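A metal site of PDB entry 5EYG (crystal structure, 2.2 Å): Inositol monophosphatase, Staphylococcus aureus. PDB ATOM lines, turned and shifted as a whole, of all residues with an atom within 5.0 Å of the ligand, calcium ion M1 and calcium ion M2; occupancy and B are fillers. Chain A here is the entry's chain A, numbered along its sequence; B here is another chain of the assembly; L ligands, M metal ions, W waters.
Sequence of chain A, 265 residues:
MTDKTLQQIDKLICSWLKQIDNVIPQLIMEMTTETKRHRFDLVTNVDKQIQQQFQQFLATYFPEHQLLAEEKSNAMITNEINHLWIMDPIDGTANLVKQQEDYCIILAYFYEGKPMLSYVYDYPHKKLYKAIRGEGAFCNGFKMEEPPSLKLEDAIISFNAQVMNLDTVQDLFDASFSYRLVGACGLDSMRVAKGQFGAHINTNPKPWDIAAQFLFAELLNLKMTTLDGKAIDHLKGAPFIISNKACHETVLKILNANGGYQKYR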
ATOM      1  N   ASP A  47       6.443  22.869  27.861  1.00  0.00           N
ATOM      2  CA  ASP A  47       7.826  22.912  28.282  1.00  0.00           C
ATOM      3  C   ASP A  47       7.938  23.538  29.690  1.00  0.00           C
ATOM      4  O   ASP A  47       8.550  22.946  30.600  1.00  0.00           O
ATOM      5  CB  ASP A  47       8.637  23.728  27.264  1.00  0.00           C
ATOM      6  CG  ASP A  47       8.420  23.268  25.785  1.00  0.00           C
ATOM      7  OD1 ASP A  47       7.272  23.291  25.269  1.00  0.00           O
ATOM      8  OD2 ASP A  47       9.408  22.893  25.157  1.00  0.00           O
ATOM      9  N   GLU A  70      16.439  23.895  30.317  1.00  0.00           N
ATOM     10  CA  GLU A  70      16.317  24.817  29.168  1.00  0.00           C
ATOM     11  C   GLU A  70      15.537  26.073  29.508  1.00  0.00           C
ATOM     12  O   GLU A  70      15.913  27.142  29.094  1.00  0.00           O
ATOM     13  CB  GLU A  70      15.737  24.124  27.910  1.00  0.00           C
ATOM     14  CG  GLU A  70      15.620  25.028  26.704  1.00  0.00           C
ATOM     15  CD  GLU A  70      15.550  24.254  25.418  1.00  0.00           C
ATOM     16  OE1 GLU A  70      15.976  24.781  24.362  1.00  0.00           O
ATOM     17  OE2 GLU A  70      15.161  23.081  25.427  1.00  0.00           O
ATOM     18  N   GLU A  71      14.483  25.975  30.285  1.00  0.00           N
ATOM     19  CA  GLU A  71      13.560  27.088  30.477  1.00  0.00           C
ATOM     20  C   GLU A  71      13.855  27.966  31.702  1.00  0.00           C
ATOM     21  O   GLU A  71      12.966  28.614  32.194  1.00  0.00           O
ATOM     22  CB  GLU A  71      12.133  26.581  30.502  1.00  0.00           C
ATOM     23  CG  GLU A  71      11.809  25.599  29.397  1.00  0.00           C
ATOM     24  CD  GLU A  71      12.014  26.204  28.000  1.00  0.00           C
ATOM     25  OE1 GLU A  71      11.983  27.465  27.856  1.00  0.00           O
ATOM     26  OE2 GLU A  71      12.214  25.414  27.050  1.00  0.00           O
ATOM     27  N   ASP A  88      15.845  18.586  29.820  1.00  0.00           N
ATOM     28  CA  ASP A  88      15.104  19.161  28.714  1.00  0.00           C
ATOM     29  C   ASP A  88      13.639  18.792  28.904  1.00  0.00           C
ATOM     30  O   ASP A  88      13.233  17.603  28.738  1.00  0.00           O
ATOM     31  CB  ASP A  88      15.627  18.707  27.383  1.00  0.00           C
ATOM     32  CG  ASP A  88      15.129  19.600  26.238  1.00  0.00           C
ATOM     33  OD1 ASP A  88      14.171  20.425  26.452  1.00  0.00           O
ATOM     34  OD2 ASP A  88      15.683  19.490  25.110  1.00  0.00           O
ATOM     35  N   PRO A  89      12.823  19.757  29.330  1.00  0.00           N
ATOM     36  CA  PRO A  89      11.448  19.329  29.707  1.00  0.00           C
ATOM     37  C   PRO A  89      10.639  18.868  28.561  1.00  0.00           C
ATOM     38  O   PRO A  89       9.812  17.965  28.758  1.00  0.00           O
ATOM     39  CB  PRO A  89      10.828  20.582  30.297  1.00  0.00           C
ATOM     40  CG  PRO A  89      11.671  21.696  29.815  1.00  0.00           C
ATOM     41  CD  PRO A  89      13.067  21.176  29.622  1.00  0.00           C
ATOM     42  N   ILE A  90      10.792  19.478  27.393  1.00  0.00           N
ATOM     43  CA  ILE A  90      10.323  18.866  26.134  1.00  0.00           C
ATOM     44  C   ILE A  90      11.452  18.965  25.131  1.00  0.00           C
ATOM     45  O   ILE A  90      11.773  20.055  24.709  1.00  0.00           O
ATOM     46  CB  ILE A  90       9.090  19.597  25.563  1.00  0.00           C
ATOM     47  CG1 ILE A  90       7.877  19.409  26.448  1.00  0.00           C
ATOM     48  CG2 ILE A  90       8.769  19.155  24.154  1.00  0.00           C
ATOM     49  CD1 ILE A  90       7.364  17.976  26.481  1.00  0.00           C
ATOM     50  N   ASP A  91      12.006  17.832  24.755  1.00  0.00           N
ATOM     51  CA  ASP A  91      12.979  17.819  23.676  1.00  0.00           C
ATOM     52  C   ASP A  91      12.220  17.410  22.440  1.00  0.00           C
ATOM     53  O   ASP A  91      11.589  16.384  22.420  1.00  0.00           O
ATOM     54  CB  ASP A  91      14.073  16.828  23.966  1.00  0.00           C
ATOM     55  CG  ASP A  91      15.042  16.737  22.815  1.00  0.00           C
ATOM     56  OD1 ASP A  91      15.517  17.805  22.374  1.00  0.00           O
ATOM     57  OD2 ASP A  91      15.300  15.636  22.399  1.00  0.00           O
ATOM     58  N   GLY A  92      12.290  18.182  21.385  1.00  0.00           N
ATOM     59  CA  GLY A  92      11.369  18.034  20.278  1.00  0.00           C
ATOM     60  C   GLY A  92      10.139  18.969  20.348  1.00  0.00           C
ATOM     61  O   GLY A  92       9.034  18.565  20.027  1.00  0.00           O
ATOM     62  N   THR A  93      10.351  20.211  20.738  1.00  0.00           N
ATOM     63  CA  THR A  93       9.268  21.176  20.886  1.00  0.00           C
ATOM     64  C   THR A  93       8.544  21.383  19.529  1.00  0.00           C
ATOM     65  O   THR A  93       7.319  21.481  19.461  1.00  0.00           O
ATOM     66  CB  THR A  93       9.828  22.518  21.398  1.00  0.00           C
ATOM     67  OG1 THR A  93      10.406  22.334  22.702  1.00  0.00           O
ATOM     68  CG2 THR A  93       8.747  23.524  21.549  1.00  0.00           C
ATOM     69  N   ALA A  94       9.322  21.410  18.459  1.00  0.00           N
ATOM     70  CA  ALA A  94       8.744  21.579  17.121  1.00  0.00           C
ATOM     71  C   ALA A  94       7.822  20.395  16.832  1.00  0.00           C
ATOM     72  O   ALA A  94       6.708  20.614  16.381  1.00  0.00           O
ATOM     73  CB  ALA A  94       9.780  21.769  16.038  1.00  0.00           C
ATOM     74  N   ASN A 160      20.759  16.588  11.099  1.00  0.00           N
ATOM     75  CA  ASN A 160      20.059  17.725  10.506  1.00  0.00           C
ATOM     76  C   ASN A 160      20.841  18.143   9.274  1.00  0.00           C
ATOM     77  O   ASN A 160      21.931  18.719   9.361  1.00  0.00           O
ATOM     78  CB  ASN A 160      19.970  18.870  11.525  1.00  0.00           C
ATOM     79  CG  ASN A 160      19.089  20.006  11.065  1.00  0.00           C
ATOM     80  OD1 ASN A 160      18.727  20.118   9.867  1.00  0.00           O
ATOM     81  ND2 ASN A 160      18.729  20.877  12.002  1.00  0.00           N
ATOM     82  N   GLN A 162      20.108  20.498   7.215  1.00  0.00           N
ATOM     83  CA  GLN A 162      19.973  21.928   6.935  1.00  0.00           C
ATOM     84  C   GLN A 162      21.065  22.797   7.550  1.00  0.00           C
ATOM     85  O   GLN A 162      21.119  23.955   7.266  1.00  0.00           O
ATOM     86  CB  GLN A 162      18.621  22.480   7.499  1.00  0.00           C
ATOM     87  CG  GLN A 162      17.421  21.608   7.136  1.00  0.00           C
ATOM     88  CD  GLN A 162      16.062  22.213   7.424  1.00  0.00           C
ATOM     89  OE1 GLN A 162      15.213  21.550   7.991  1.00  0.00           O
ATOM     90  NE2 GLN A 162      15.832  23.410   7.005  1.00  0.00           N
ATOM     91  N   VAL A 163      21.958  22.188   8.344  1.00  0.00           N
ATOM     92  CA  VAL A 163      22.987  22.965   9.024  1.00  0.00           C
ATOM     93  C   VAL A 163      24.355  22.583   8.545  1.00  0.00           C
ATOM     94  O   VAL A 163      25.313  22.937   9.178  1.00  0.00           O
ATOM     95  CB  VAL A 163      22.944  22.877  10.563  1.00  0.00           C
ATOM     96  CG1 VAL A 163      21.669  23.510  11.074  1.00  0.00           C
ATOM     97  CG2 VAL A 163      23.222  21.466  11.087  1.00  0.00           C
ATOM     98  N   GLY A 183      13.695  13.904  14.758  1.00  0.00           N
ATOM     99  CA  GLY A 183      13.623  15.362  15.018  1.00  0.00           C
ATOM    100  C   GLY A 183      13.640  15.697  16.506  1.00  0.00           C
ATOM    101  O   GLY A 183      13.387  16.862  16.859  1.00  0.00           O
ATOM    102  N   ALA A 184      13.909  14.723  17.346  1.00  0.00           N
ATOM    103  CA  ALA A 184      14.227  15.051  18.743  1.00  0.00           C
ATOM    104  C   ALA A 184      15.503  14.354  19.133  1.00  0.00           C
ATOM    105  O   ALA A 184      15.626  13.151  19.038  1.00  0.00           O
ATOM    106  CB  ALA A 184      13.089  14.593  19.626  1.00  0.00           C
ATOM    107  N   CYS A 185      16.484  15.134  19.584  1.00  0.00           N
ATOM    108  CA  CYS A 185      17.813  14.589  19.961  1.00  0.00           C
ATOM    109  C   CYS A 185      17.730  13.356  20.806  1.00  0.00           C
ATOM    110  O   CYS A 185      18.427  12.359  20.528  1.00  0.00           O
ATOM    111  CB  CYS A 185      18.688  15.671  20.638  1.00  0.00           C
ATOM    112  SG  CYS A 185      20.403  15.170  20.707  1.00  0.00           S
ATOM    113  N   ILE A 201      23.784  12.675  14.782  1.00  0.00           N
ATOM    114  CA  ILE A 201      24.644  13.838  14.953  1.00  0.00           C
ATOM    115  C   ILE A 201      23.854  15.102  15.257  1.00  0.00           C
ATOM    116  O   ILE A 201      22.792  15.346  14.660  1.00  0.00           O
ATOM    117  CB  ILE A 201      25.386  14.128  13.608  1.00  0.00           C
ATOM    118  CG1 ILE A 201      26.219  12.925  13.192  1.00  0.00           C
ATOM    119  CG2 ILE A 201      26.269  15.386  13.746  1.00  0.00           C
ATOM    120  CD1 ILE A 201      26.426  12.809  11.676  1.00  0.00           C
ATOM    121  N   ASN A 202      24.363  15.885  16.196  1.00  0.00           N
ATOM    122  CA  ASN A 202      23.843  17.244  16.347  1.00  0.00           C
ATOM    123  C   ASN A 202      25.014  18.178  16.480  1.00  0.00           C
ATOM    124  O   ASN A 202      25.800  18.039  17.443  1.00  0.00           O
ATOM    125  CB  ASN A 202      22.964  17.359  17.598  1.00  0.00           C
ATOM    126  CG  ASN A 202      22.347  18.761  17.781  1.00  0.00           C
ATOM    127  OD1 ASN A 202      23.024  19.813  17.650  1.00  0.00           O
ATOM    128  ND2 ASN A 202      21.068  18.789  18.099  1.00  0.00           N
ATOM    129  N   THR A 203      25.169  19.088  15.530  1.00  0.00           N
ATOM    130  CA  THR A 203      26.390  19.905  15.435  1.00  0.00           C
ATOM    131  C   THR A 203      26.437  21.020  16.424  1.00  0.00           C
ATOM    132  O   THR A 203      27.445  21.692  16.501  1.00  0.00           O
ATOM    133  CB  THR A 203      26.605  20.456  14.034  1.00  0.00           C
ATOM    134  OG1 THR A 203      25.514  21.278  13.701  1.00  0.00           O
ATOM    135  CG2 THR A 203      26.694  19.311  13.015  1.00  0.00           C
ATOM    136  N   ASN A 204      25.391  21.238  17.203  1.00  0.00           N
ATOM    137  CA  ASN A 204      25.454  22.298  18.180  1.00  0.00           C
ATOM    138  C   ASN A 204      24.462  22.147  19.325  1.00  0.00           C
ATOM    139  O   ASN A 204      23.533  22.971  19.485  1.00  0.00           O
ATOM    140  CB  ASN A 204      25.206  23.611  17.474  1.00  0.00           C
ATOM    141  CG  ASN A 204      25.607  24.781  18.294  1.00  0.00           C
ATOM    142  OD1 ASN A 204      26.320  24.682  19.307  1.00  0.00           O
ATOM    143  ND2 ASN A 204      25.093  25.925  17.904  1.00  0.00           N
ATOM    144  N   PRO A 205      24.622  21.065  20.110  1.00  0.00           N
ATOM    145  CA  PRO A 205      23.630  20.830  21.148  1.00  0.00           C
ATOM    146  C   PRO A 205      23.845  21.646  22.418  1.00  0.00           C
ATOM    147  O   PRO A 205      24.977  22.005  22.747  1.00  0.00           O
ATOM    148  CB  PRO A 205      23.820  19.363  21.466  1.00  0.00           C
ATOM    149  CG  PRO A 205      25.268  19.110  21.180  1.00  0.00           C
ATOM    150  CD  PRO A 205      25.580  19.973  19.990  1.00  0.00           C
ATOM    151  N   TRP A 208      21.270  20.057  27.871  1.00  0.00           N
ATOM    152  CA  TRP A 208      20.049  19.314  28.074  1.00  0.00           C
ATOM    153  C   TRP A 208      19.662  18.388  26.894  1.00  0.00           C
ATOM    154  O   TRP A 208      18.933  17.457  27.109  1.00  0.00           O
ATOM    155  CB  TRP A 208      18.889  20.229  28.459  1.00  0.00           C
ATOM    156  CG  TRP A 208      18.771  21.471  27.626  1.00  0.00           C
ATOM    157  CD1 TRP A 208      18.178  21.605  26.400  1.00  0.00           C
ATOM    158  CD2 TRP A 208      19.313  22.733  27.940  1.00  0.00           C
ATOM    159  NE1 TRP A 208      18.311  22.891  25.938  1.00  0.00           N
ATOM    160  CE2 TRP A 208      19.015  23.604  26.862  1.00  0.00           C
ATOM    161  CE3 TRP A 208      20.026  23.217  29.032  1.00  0.00           C
ATOM    162  CZ2 TRP A 208      19.362  24.951  26.866  1.00  0.00           C
ATOM    163  CZ3 TRP A 208      20.381  24.563  29.043  1.00  0.00           C
ATOM    164  CH2 TRP A 208      20.064  25.416  27.955  1.00  0.00           C
ATOM    165  N   ASP A 209      20.091  18.712  25.676  1.00  0.00           N
ATOM    166  CA  ASP A 209      19.843  17.875  24.527  1.00  0.00           C
ATOM    167  C   ASP A 209      20.557  16.528  24.634  1.00  0.00           C
ATOM    168  O   ASP A 209      20.062  15.567  24.059  1.00  0.00           O
ATOM    169  CB  ASP A 209      20.392  18.520  23.265  1.00  0.00           C
ATOM    170  CG  ASP A 209      19.642  19.759  22.864  1.00  0.00           C
ATOM    171  OD1 ASP A 209      18.389  19.736  22.946  1.00  0.00           O
ATOM    172  OD2 ASP A 209      20.320  20.739  22.445  1.00  0.00           O
ATOM    173  N   PHE B 177       8.831  24.782   7.321  1.00  0.00           N
ATOM    174  CA  PHE B 177       9.145  24.997   8.707  1.00  0.00           C
ATOM    175  C   PHE B 177      10.252  24.090   9.138  1.00  0.00           C
ATOM    176  O   PHE B 177      11.182  24.505   9.799  1.00  0.00           O
ATOM    177  CB  PHE B 177       7.924  24.777   9.568  1.00  0.00           C
ATOM    178  CG  PHE B 177       8.180  25.088  10.975  1.00  0.00           C
ATOM    179  CD1 PHE B 177       8.080  26.389  11.445  1.00  0.00           C
ATOM    180  CD2 PHE B 177       8.571  24.092  11.835  1.00  0.00           C
ATOM    181  CE1 PHE B 177       8.341  26.669  12.761  1.00  0.00           C
ATOM    182  CE2 PHE B 177       8.852  24.398  13.146  1.00  0.00           C
ATOM    183  CZ  PHE B 177       8.730  25.672  13.607  1.00  0.00           C
ATOM    184  N   SER B 178      10.176  22.833   8.753  1.00  0.00           N
ATOM    185  CA  SER B 178      11.240  21.863   9.002  1.00  0.00           C
ATOM    186  C   SER B 178      11.071  20.611   8.134  1.00  0.00           C
ATOM    187  O   SER B 178      10.157  20.496   7.332  1.00  0.00           O
ATOM    188  CB  SER B 178      11.278  21.466  10.477  1.00  0.00           C
ATOM    189  OG  SER B 178      12.513  20.819  10.797  1.00  0.00           O
ATOM    190  N   ARG B 180      11.334  16.237   8.056  1.00  0.00           N
ATOM    191  CA  ARG B 180      11.337  14.968   8.821  1.00  0.00           C
ATOM    192  C   ARG B 180      11.178  13.852   7.811  1.00  0.00           C
ATOM    193  O   ARG B 180      10.720  14.070   6.653  1.00  0.00           O
ATOM    194  CB  ARG B 180      10.204  14.889   9.815  1.00  0.00           C
ATOM    195  CG  ARG B 180      10.076  15.947  10.904  1.00  0.00           C
ATOM    196  CD  ARG B 180      10.679  15.750  12.320  1.00  0.00           C
ATOM    197  NE  ARG B 180      11.670  16.664  12.321  1.00  0.00           N
ATOM    198  CZ  ARG B 180      11.801  17.901  12.715  1.00  0.00           C
ATOM    199  NH1 ARG B 180      11.363  18.469  13.824  1.00  0.00           N
ATOM    200  NH2 ARG B 180      12.855  18.378  12.121  1.00  0.00           N
HETATM  201  P1  LIG L   1      14.299  21.280  15.511  1.00  0.00           P
HETATM  202  O1  LIG L   1      13.810  20.324  14.441  1.00  0.00           O
HETATM  203  O2  LIG L   1      13.405  22.334  16.048  1.00  0.00           O
HETATM  204  O3  LIG L   1      14.898  20.407  16.740  1.00  0.00           O
HETATM  205  C1  LIG L   1      15.721  19.317  16.402  1.00  0.00           C
HETATM  206  C2  LIG L   1      16.477  18.876  17.638  1.00  0.00           C
HETATM  207  O4  LIG L   1      17.615  19.721  17.833  1.00  0.00           O
HETATM  208  C3  LIG L   1      15.627  18.890  18.951  1.00  0.00           C
HETATM  209  O5  LIG L   1      16.202  17.977  19.865  1.00  0.00           O
HETATM  210  C4  LIG L   1      15.838  20.300  19.463  1.00  0.00           C
HETATM  211  O6  LIG L   1      15.728  20.528  20.870  1.00  0.00           O
HETATM  212  C5  LIG L   1      17.298  20.527  18.998  1.00  0.00           C
HETATM  213  N1  LIG L   1      17.596  21.944  18.716  1.00  0.00           N
HETATM  214  C6  LIG L   1      16.760  23.012  18.743  1.00  0.00           C
HETATM  215  N2  LIG L   1      17.486  24.135  18.412  1.00  0.00           N
HETATM  216  C7  LIG L   1      18.747  23.770  18.168  1.00  0.00           C
HETATM  217  C8  LIG L   1      19.991  24.447  17.781  1.00  0.00           C
HETATM  218  N3  LIG L   1      19.957  25.746  17.599  1.00  0.00           N
HETATM  219  N4  LIG L   1      21.106  23.776  17.569  1.00  0.00           N
HETATM  220  C9  LIG L   1      21.062  22.434  17.780  1.00  0.00           C
HETATM  221  N5  LIG L   1      19.974  21.705  18.157  1.00  0.00           N
HETATM  222  C10 LIG L   1      18.811  22.332  18.344  1.00  0.00           C
HETATM  223  O7  LIG L   1      15.627  21.813  14.803  1.00  0.00           O
HETATM  224  P2  LIG L   1      15.425  22.739  13.464  1.00  0.00           P
HETATM  225  O8  LIG L   1      14.289  22.137  12.683  1.00  0.00           O
HETATM  226  O9  LIG L   1      16.702  22.941  12.726  1.00  0.00           O
HETATM  227  O10 LIG L   1      15.072  24.103  14.329  1.00  0.00           O
HETATM  228  C11 LIG L   1      15.306  25.492  14.045  1.00  0.00           C
HETATM  229  C12 LIG L   1      16.776  25.863  14.254  1.00  0.00           C
HETATM  230  O11 LIG L   1      17.453  24.900  15.079  1.00  0.00           O
HETATM  231  C13 LIG L   1      17.506  25.889  12.905  1.00  0.00           C
HETATM  232  O12 LIG L   1      17.628  27.229  12.446  1.00  0.00           O
HETATM  233  C14 LIG L   1      18.836  25.099  13.116  1.00  0.00           C
HETATM  234  O13 LIG L   1      20.052  25.831  12.887  1.00  0.00           O
HETATM  235  C15 LIG L   1      18.788  24.583  14.570  1.00  0.00           C
HETATM  236  N6  LIG L   1      19.192  23.135  14.700  1.00  0.00           N
HETATM  237  C16 LIG L   1      20.489  22.737  14.504  1.00  0.00           C
HETATM  238  C17 LIG L   1      20.872  21.364  14.623  1.00  0.00           C
HETATM  239  C18 LIG L   1      22.295  20.893  14.451  1.00  0.00           C
HETATM  240  O14 LIG L   1      22.540  19.677  14.182  1.00  0.00           O
HETATM  241  N7  LIG L   1      23.250  21.857  14.668  1.00  0.00           N
HETATM  242  C19 LIG L   1      19.910  20.413  14.986  1.00  0.00           C
HETATM  243  C20 LIG L   1      18.611  20.841  15.173  1.00  0.00           C
HETATM  244  C21 LIG L   1      18.272  22.193  15.028  1.00  0.00           C
HETATM  245  P3  LIG L   1      14.339  21.253  21.360  1.00  0.00           P
HETATM  246  O15 LIG L   1      13.181  20.629  20.620  1.00  0.00           O
HETATM  247  O16 LIG L   1      14.249  21.037  22.859  1.00  0.00           O
HETATM  248  O17 LIG L   1      14.472  22.646  20.845  1.00  0.00           O
HETATM  249 CA    CA M   1      13.415  21.727  24.750  1.00  0.00          CA
HETATM  250 CA    CA M   2      16.317  19.855  23.051  1.00  0.00          CA
HETATM  251  O   HOH W   1      17.330  22.216  23.386  1.00  0.00           O
HETATM  252  O   HOH W   2      15.655  24.713  21.884  1.00  0.00           O
HETATM  253  O   HOH W   3      11.984  22.808  26.154  1.00  0.00           O
HETATM  254  O   HOH W   4      12.583  23.421  23.312  1.00  0.00           O
HETATM  255  O   HOH W   5      20.742  17.172  14.583  1.00  0.00           O
HETATM  256  O   HOH W   6      17.411  23.968  10.565  1.00  0.00           O
HETATM  257  O   HOH W   7      23.261  17.580  12.159  1.00  0.00           O
HETATM  258  O   HOH W   8      19.166  23.128  21.530  1.00  0.00           O
HETATM  259  O   HOH W   9      12.120  21.209  18.247  1.00  0.00           O
HETATM  260  O   HOH W  10      15.807  19.391  12.595  1.00  0.00           O
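ND2 of Asn 160 lies within hydrogen-bond range of O9 of the ligand (3.0 Å).
ND2 of Asn 202 lies within hydrogen-bond range of N5 of the ligand (3.1 Å).
An oxygen (O1) of the ligand lies within salt-bridge range of the guanidinium group (NH1) of Arg 180 of chain B (3.1 Å).
N of Thr 93 sits at hydrogen-bond distance from O15 of the ligand, at 2.9 Å.
An oxygen (O5) of the ligand sits at hydrogen-bond distance from the backbone NH (N) of Cys 185.
N of Gly 92 lies within hydrogen-bond range of O15 of the ligand (2.7 Å).
OG of Ser 178 of chain B lies within hydrogen-bond range of O8 of the ligand (2.9 Å).
An oxygen (O14) of the ligand is in hydrogen-bond range of the backbone NH of Thr 203 (3.0 Å).
OG1 of Thr 203 sits at hydrogen-bond distance from N7 of the ligand, at 2.5 Å.
The side-chain amide oxygen of Asn 160 lies within hydrogen-bond range of the backbone NH of Gln 162 (3.0 Å).
The backbone NH (N) of Asn 204 lies within hydrogen-bond range of the side-chain amide oxygen (OD1) of Asn 202 (2.8 Å).
The guanidinium group of Arg 180 of chain B sits at hydrogen-bond distance from the side-chain hydroxyl of Ser 178 of chain B, at 2.8 Å.
O of Asp 209 is in hydrogen-bond range of SG of Cys 185 (3.4 Å).
The side-chain carboxylate of Asp 91 sits at hydrogen-bond distance from the backbone NH of Cys 185 (3.1 Å).
OD2 of Asp 47 is in hydrogen-bond range of OG1 of Thr 93 (2.7 Å).
The indole nitrogen (NE1) of Trp 208 lies close to the side-chain carboxylate (OE1) of Glu 70, 3.4 Å away.
O of Ile 90 sits close to OG1 of Thr 93.
The backbone carbonyl oxygen (O) of Asn 204 sits close to a nitrogen (N4) of the ligand (3.2 Å).
Residues that only touch the ligand: Val 163 (3.4 Å), Gly 183 (3.4 Å), Ala 94 (3.7 Å) and Ala 184 (3.7 Å).
Of the 26 residues printed, 18 come within 4 Å of the ligand.
The nearest printed residue that does not touch the ligand is Ile 201 (4.4 Å).
Residues that only touch calcium ion M1: Thr 93 (3.7 Å).
Four residues have an atom within 4 Å of calcium ion M1: Glu 70, Asp 88, Ile 90 and Thr 93.
The nearest printed residue that does not touch calcium ion M2 is Glu 70 (4.2 Å).
Calcium ion M1 is bound by O16 of the ligand (2.2 Å), OD1 of Asp 88 (2.3 Å), water W3 (2.3 Å), OE2 of Glu 70 (2.3 Å), O of Ile 90 (2.3 Å) and water W4 (2.4 Å).
Calcium ion M1 has six donor atoms within binding distance.
Calcium ion M2 is bound by OD1 of Asp 209 (2.1 Å), OD2 of Asp 88 (2.2 Å), OD1 of Asp 91 (2.3 Å), O6 of the ligand (2.4 Å), O16 of the ligand (2.4 Å) and water W1 (2.6 Å).
Water W4 lies within hydrogen-bond range of the side-chain hydroxyl of Thr 93 (2.5 Å) and an oxygen (O17) of the ligand (3.2 Å).
Water W3 lies within hydrogen-bond range of OD2 of Asp 47 (2.8 Å) and OE2 of Glu 71 (2.8 Å).
Water W2 bridges OE1 of Glu 70 (2.5 Å) and O17 of the ligand (2.6 Å).
Water W9 lies within hydrogen-bond range of an oxygen (O15) of the ligand, the backbone NH of Ala 94 and the backbone NH of Thr 93.
Water W10 lies within hydrogen-bond range of O1 of the ligand (2.9 Å), NH2 of Arg 180 of chain B (3.2 Å) and ND2 of Asn 160 (3.3 Å).
Water W5 lies within hydrogen-bond range of O of Ile 201 (2.7 Å) and O14 of the ligand (3.1 Å).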
